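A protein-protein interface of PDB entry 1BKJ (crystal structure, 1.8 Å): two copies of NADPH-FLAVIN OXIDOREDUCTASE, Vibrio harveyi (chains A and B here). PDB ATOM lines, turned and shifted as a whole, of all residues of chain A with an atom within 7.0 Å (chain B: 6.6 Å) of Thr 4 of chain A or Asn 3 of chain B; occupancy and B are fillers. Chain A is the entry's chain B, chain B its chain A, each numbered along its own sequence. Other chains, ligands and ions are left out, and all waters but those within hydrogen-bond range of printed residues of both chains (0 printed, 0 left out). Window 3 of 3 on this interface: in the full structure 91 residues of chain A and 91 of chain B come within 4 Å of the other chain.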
ATOM      1  N   ASN A   2     -17.104  16.216 -18.313  1.00  0.00           N
ATOM      2  CA  ASN A   2     -16.148  15.281 -17.728  1.00  0.00           C
ATOM      3  C   ASN A   2     -14.723  15.811 -17.812  1.00  0.00           C
ATOM      4  O   ASN A   2     -14.459  16.773 -18.535  1.00  0.00           O
ATOM      5  CB  ASN A   2     -16.280  13.876 -18.361  1.00  0.00           C
ATOM      6  CG  ASN A   2     -15.974  13.843 -19.869  1.00  0.00           C
ATOM      7  OD1 ASN A   2     -14.827  14.004 -20.281  1.00  0.00           O
ATOM      8  ND2 ASN A   2     -16.998  13.565 -20.683  1.00  0.00           N
ATOM      9  N   ASN A   3     -13.803  15.149 -17.114  1.00  0.00           N
ATOM     10  CA  ASN A   3     -12.403  15.567 -17.066  1.00  0.00           C
ATOM     11  C   ASN A   3     -11.570  15.510 -18.359  1.00  0.00           C
ATOM     12  O   ASN A   3     -10.738  16.397 -18.562  1.00  0.00           O
ATOM     13  CB  ASN A   3     -11.667  14.862 -15.915  1.00  0.00           C
ATOM     14  N   THR A   4     -11.803  14.518 -19.231  1.00  0.00           N
ATOM     15  CA  THR A   4     -11.056  14.390 -20.504  1.00  0.00           C
ATOM     16  C   THR A   4     -11.335  15.571 -21.440  1.00  0.00           C
ATOM     17  O   THR A   4     -10.411  16.120 -22.042  1.00  0.00           O
ATOM     18  CB  THR A   4     -11.388  13.065 -21.246  1.00  0.00           C
ATOM     19  OG1 THR A   4     -11.137  11.953 -20.379  1.00  0.00           O
ATOM     20  CG2 THR A   4     -10.559  12.878 -22.526  1.00  0.00           C
ATOM     21  N   ILE A   5     -12.599  15.984 -21.496  1.00  0.00           N
ATOM     22  CA  ILE A   5     -13.044  17.094 -22.334  1.00  0.00           C
ATOM     23  C   ILE A   5     -12.547  18.438 -21.788  1.00  0.00           C
ATOM     24  O   ILE A   5     -12.128  19.302 -22.570  1.00  0.00           O
ATOM     25  CB  ILE A   5     -14.586  17.040 -22.532  1.00  0.00           C
ATOM     26  CG1 ILE A   5     -14.922  15.813 -23.376  1.00  0.00           C
ATOM     27  CG2 ILE A   5     -15.111  18.286 -23.257  1.00  0.00           C
ATOM     28  CD1 ILE A   5     -16.372  15.519 -23.462  1.00  0.00           C
ATOM     29  N   GLU A   6     -12.517  18.571 -20.458  1.00  0.00           N
ATOM     30  CA  GLU A   6     -12.040  19.790 -19.782  1.00  0.00           C
ATOM     31  C   GLU A   6     -10.533  19.998 -20.042  1.00  0.00           C
ATOM     32  O   GLU A   6     -10.103  21.123 -20.315  1.00  0.00           O
ATOM     33  CB  GLU A   6     -12.351  19.734 -18.278  1.00  0.00           C
ATOM     34  N   THR A   7      -9.776  18.895 -20.082  1.00  0.00           N
ATOM     35  CA  THR A   7      -8.324  18.904 -20.354  1.00  0.00           C
ATOM     36  C   THR A   7      -8.047  19.273 -21.826  1.00  0.00           C
ATOM     37  O   THR A   7      -7.170  20.105 -22.107  1.00  0.00           O
ATOM     38  CB  THR A   7      -7.676  17.522 -20.035  1.00  0.00           C
ATOM     39  OG1 THR A   7      -7.886  17.208 -18.654  1.00  0.00           O
ATOM     40  CG2 THR A   7      -6.165  17.516 -20.324  1.00  0.00           C
ATOM     41  N   ILE A   8      -8.806  18.663 -22.744  1.00  0.00           N
ATOM     42  CA  ILE A   8      -8.674  18.921 -24.179  1.00  0.00           C
ATOM     43  C   ILE A   8      -8.915  20.396 -24.512  1.00  0.00           C
ATOM     44  O   ILE A   8      -8.085  21.007 -25.182  1.00  0.00           O
ATOM     45  CB  ILE A   8      -9.636  18.036 -25.023  1.00  0.00           C
ATOM     46  CG1 ILE A   8      -9.210  16.569 -24.956  1.00  0.00           C
ATOM     47  CG2 ILE A   8      -9.631  18.475 -26.484  1.00  0.00           C
ATOM     48  CD1 ILE A   8     -10.188  15.588 -25.606  1.00  0.00           C
ATOM     49  N   LEU A   9     -10.018  20.962 -24.007  1.00  0.00           N
ATOM     50  CA  LEU A   9     -10.378  22.365 -24.273  1.00  0.00           C
ATOM     51  C   LEU A   9      -9.522  23.418 -23.560  1.00  0.00           C
ATOM     52  O   LEU A   9      -9.502  24.581 -23.965  1.00  0.00           O
ATOM     53  CB  LEU A   9     -11.862  22.596 -23.965  1.00  0.00           C
ATOM     54  CG  LEU A   9     -12.920  21.783 -24.733  1.00  0.00           C
ATOM     55  CD1 LEU A   9     -14.316  22.045 -24.162  1.00  0.00           C
ATOM     56  CD2 LEU A   9     -12.893  22.135 -26.208  1.00  0.00           C
ATOM     57  N   LEU A 117      -1.795  14.915 -24.227  1.00  0.00           N
ATOM     58  CA  LEU A 117      -3.000  14.934 -23.395  1.00  0.00           C
ATOM     59  C   LEU A 117      -2.797  14.287 -22.051  1.00  0.00           C
ATOM     60  O   LEU A 117      -3.326  14.770 -21.058  1.00  0.00           O
ATOM     61  CB  LEU A 117      -4.196  14.295 -24.088  1.00  0.00           C
ATOM     62  CG  LEU A 117      -4.918  15.283 -25.003  1.00  0.00           C
ATOM     63  CD1 LEU A 117      -5.951  14.552 -25.804  1.00  0.00           C
ATOM     64  CD2 LEU A 117      -5.555  16.415 -24.193  1.00  0.00           C
ATOM     65  N   SER A 121      -2.954  16.457 -18.500  1.00  0.00           N
ATOM     66  CA  SER A 121      -3.895  16.035 -17.457  1.00  0.00           C
ATOM     67  C   SER A 121      -3.246  15.886 -16.081  1.00  0.00           C
ATOM     68  O   SER A 121      -3.946  15.886 -15.068  1.00  0.00           O
ATOM     69  CB  SER A 121      -4.580  14.730 -17.839  1.00  0.00           C
ATOM     70  OG  SER A 121      -3.684  13.640 -17.843  1.00  0.00           O
ATOM     71  N   ASN B   2      -6.132   9.728 -13.207  1.00  0.00           N
ATOM     72  CA  ASN B   2      -7.243  10.619 -13.552  1.00  0.00           C
ATOM     73  C   ASN B   2      -8.119  10.029 -14.657  1.00  0.00           C
ATOM     74  O   ASN B   2      -7.724   9.030 -15.278  1.00  0.00           O
ATOM     75  CB  ASN B   2      -6.735  12.031 -13.928  1.00  0.00           C
ATOM     76  CG  ASN B   2      -5.714  12.030 -15.070  1.00  0.00           C
ATOM     77  OD1 ASN B   2      -6.064  11.833 -16.224  1.00  0.00           O
ATOM     78  ND2 ASN B   2      -4.456  12.294 -14.745  1.00  0.00           N
ATOM     79  N   ASN B   3      -9.273  10.661 -14.926  1.00  0.00           N
ATOM     80  CA  ASN B   3     -10.212  10.171 -15.945  1.00  0.00           C
ATOM     81  C   ASN B   3      -9.690  10.235 -17.371  1.00  0.00           C
ATOM     82  O   ASN B   3     -10.076   9.394 -18.181  1.00  0.00           O
ATOM     83  CB  ASN B   3     -11.582  10.863 -15.859  1.00  0.00           C
ATOM     84  N   THR B   4      -8.798  11.199 -17.656  1.00  0.00           N
ATOM     85  CA  THR B   4      -8.204  11.380 -18.997  1.00  0.00           C
ATOM     86  C   THR B   4      -7.294  10.213 -19.372  1.00  0.00           C
ATOM     87  O   THR B   4      -7.401   9.675 -20.479  1.00  0.00           O
ATOM     88  CB  THR B   4      -7.401  12.712 -19.109  1.00  0.00           C
ATOM     89  OG1 THR B   4      -8.212  13.812 -18.683  1.00  0.00           O
ATOM     90  CG2 THR B   4      -6.923  12.987 -20.543  1.00  0.00           C
ATOM     91  N   ILE B   5      -6.424   9.814 -18.444  1.00  0.00           N
ATOM     92  CA  ILE B   5      -5.501   8.706 -18.676  1.00  0.00           C
ATOM     93  C   ILE B   5      -6.236   7.356 -18.708  1.00  0.00           C
ATOM     94  O   ILE B   5      -5.925   6.522 -19.557  1.00  0.00           O
ATOM     95  CB  ILE B   5      -4.284   8.758 -17.691  1.00  0.00           C
ATOM     96  CG1 ILE B   5      -3.447  10.000 -18.012  1.00  0.00           C
ATOM     97  CG2 ILE B   5      -3.369   7.547 -17.872  1.00  0.00           C
ATOM     98  CD1 ILE B   5      -2.438  10.370 -16.961  1.00  0.00           C
ATOM     99  N   GLU B   6      -7.267   7.194 -17.870  1.00  0.00           N
ATOM    100  CA  GLU B   6      -8.080   5.962 -17.825  1.00  0.00           C
ATOM    101  C   GLU B   6      -8.829   5.772 -19.158  1.00  0.00           C
ATOM    102  O   GLU B   6      -8.912   4.652 -19.662  1.00  0.00           O
ATOM    103  CB  GLU B   6      -9.069   5.978 -16.651  1.00  0.00           C
ATOM    104  N   THR B   7      -9.268   6.884 -19.761  1.00  0.00           N
ATOM    105  CA  THR B   7      -9.965   6.889 -21.047  1.00  0.00           C
ATOM    106  C   THR B   7      -8.994   6.503 -22.184  1.00  0.00           C
ATOM    107  O   THR B   7      -9.307   5.616 -22.989  1.00  0.00           O
ATOM    108  CB  THR B   7     -10.633   8.264 -21.312  1.00  0.00           C
ATOM    109  OG1 THR B   7     -11.656   8.489 -20.332  1.00  0.00           O
ATOM    110  CG2 THR B   7     -11.259   8.332 -22.694  1.00  0.00           C
ATOM    111  N   ILE B   8      -7.811   7.127 -22.206  1.00  0.00           N
ATOM    112  CA  ILE B   8      -6.775   6.843 -23.219  1.00  0.00           C
ATOM    113  C   ILE B   8      -6.372   5.355 -23.206  1.00  0.00           C
ATOM    114  O   ILE B   8      -6.314   4.708 -24.255  1.00  0.00           O
ATOM    115  CB  ILE B   8      -5.494   7.746 -23.030  1.00  0.00           C
ATOM    116  CG1 ILE B   8      -5.806   9.207 -23.394  1.00  0.00           C
ATOM    117  CG2 ILE B   8      -4.343   7.254 -23.936  1.00  0.00           C
ATOM    118  CD1 ILE B   8      -4.683  10.214 -23.090  1.00  0.00           C
ATOM    119  N   LEU B 117     -11.109  10.773 -28.644  1.00  0.00           N
ATOM    120  CA  LEU B 117     -10.988  10.771 -27.182  1.00  0.00           C
ATOM    121  C   LEU B 117     -12.183  11.440 -26.494  1.00  0.00           C
ATOM    122  O   LEU B 117     -12.702  10.918 -25.503  1.00  0.00           O
ATOM    123  CB  LEU B 117      -9.679  11.411 -26.724  1.00  0.00           C
ATOM    124  CG  LEU B 117      -8.420  10.566 -26.885  1.00  0.00           C
ATOM    125  CD1 LEU B 117      -7.235  11.378 -26.426  1.00  0.00           C
ATOM    126  CD2 LEU B 117      -8.508   9.269 -26.090  1.00  0.00           C
ATOM    127  N   ALA B 118     -12.660  12.546 -27.062  1.00  0.00           N
ATOM    128  CA  ALA B 118     -13.834  13.246 -26.536  1.00  0.00           C
ATOM    129  C   ALA B 118     -15.029  12.282 -26.598  1.00  0.00           C
ATOM    130  O   ALA B 118     -15.708  12.077 -25.598  1.00  0.00           O
ATOM    131  CB  ALA B 118     -14.129  14.486 -27.353  1.00  0.00           C
ATOM    132  N   SER B 121     -14.743   9.368 -24.020  1.00  0.00           N
ATOM    133  CA  SER B 121     -14.955   9.850 -22.658  1.00  0.00           C
ATOM    134  C   SER B 121     -16.432   9.986 -22.295  1.00  0.00           C
ATOM    135  O   SER B 121     -16.778  10.011 -21.112  1.00  0.00           O
ATOM    136  CB  SER B 121     -14.258  11.185 -22.452  1.00  0.00           C
ATOM    137  OG  SER B 121     -14.951  12.260 -23.055  1.00  0.00           O
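OG1 of Thr 4 of chain B touches O of Asn 3 of chain A, 3.6 Å away.
Thr 4 of chain A touches Asn 3 of chain B (OG1 to O, 3.5 Å).
Thr 4 of chain A touches Thr 4 of chain B.
Thr 4 of chain A touches Thr 7 of chain B (OG1 to OG1, 3.5 Å).
Thr 4 of chain A touches Ser 121 of chain B (CB to CB, 3.6 Å).
OG of Ser 121 of chain B touches CG1 of Ile 5 of chain A, 3.6 Å away.
Leu 117 of chain A touches Leu 117 of chain B (CD1 to CD1, 3.5 Å).
Thr 4 of chain B touches Ser 121 of chain A.
OG of Ser 121 of chain A touches CD1 of Ile 5 of chain B (3.6 Å).
Of the 10 printed residues of chain A, 7 touch a printed residue of chain B.
Printed residues of chain B that touch a printed residue of chain A: Asn 2, Asn 3, Thr 4, Ile 5, Thr 7, Leu 117 and Ser 121.
Among the printed residues, no Asp or Glu carboxylate lies within 4 Å of a Lys or Arg side-chain nitrogen of the other chain.
Thr 4 of chain A touches four residues of chain B.
Printed residues of chain B within 4 Å of Ser 121 of chain A: Asn 2, Thr 4 and Ile 5.
Of the printed residues of chain A, Asn 3 of chain B touches Thr 4 (3.5 Å).
Printed residues of chain A within 4 Å of Thr 7 of chain B: Thr 4.
The nearest printed residue of chain A that does not touch Asn 3 of chain B is Asn 3 of chain A (4.0003 Å).
The side-chain hydroxyl (OG) of Ser 121 of chain A is in hydrogen-bond range of the backbone carbonyl oxygen (O) of Leu 117 of chain A, at 3.4 Å.
The backbone carbonyl oxygen (O) of Asn 3 of chain B lies within hydrogen-bond range of the side-chain hydroxyl (OG1) of Thr 7 of chain B, at 2.8 Å.
The backbone NH (N) of Thr 4 of chain A lies within hydrogen-bond range of the side-chain amide oxygen (OD1) of Asn 2 of chain A (3.2 Å).
N of Thr 4 of chain B sits at hydrogen-bond distance from OD1 of Asn 2 of chain B.
OD1 of Asn 2 of chain B sits at hydrogen-bond distance from N of Ile 5 of chain B (3.0 Å).
The backbone NH (N) of Ile 5 of chain A lies within hydrogen-bond range of the side-chain amide oxygen (OD1) of Asn 2 of chain A, 3.2 Å away.
Asn 2 of chain A touches Ser 121 of chain B, and with the chains exchanged Ser 121 of chain A touches Asn 2 of chain B.
Asn 3 of chain A touches Thr 4 of chain B, and with the chains exchanged Thr 4 of chain A touches Asn 3 of chain B.
Thr 4 of chain A touches Thr 7 of chain B, and with the chains exchanged Thr 7 of chain A touches Thr 4 of chain B.
Thr 4 of chain A touches Ser 121 of chain B, and with the chains exchanged Ser 121 of chain A touches Thr 4 of chain B.
The side-chain hydroxyl of Ser 121 of chain B sits at hydrogen-bond distance from the side-chain amide oxygen of Asn 2 of chain A (3.3 Å).
The side-chain hydroxyl (OG) of Ser 121 of chain A sits at hydrogen-bond distance from the side-chain amide oxygen (OD1) of Asn 2 of chain B (3.4 Å).
OG1 of Thr 4 of chain B is in hydrogen-bond range of OG1 of Thr 7 of chain A.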
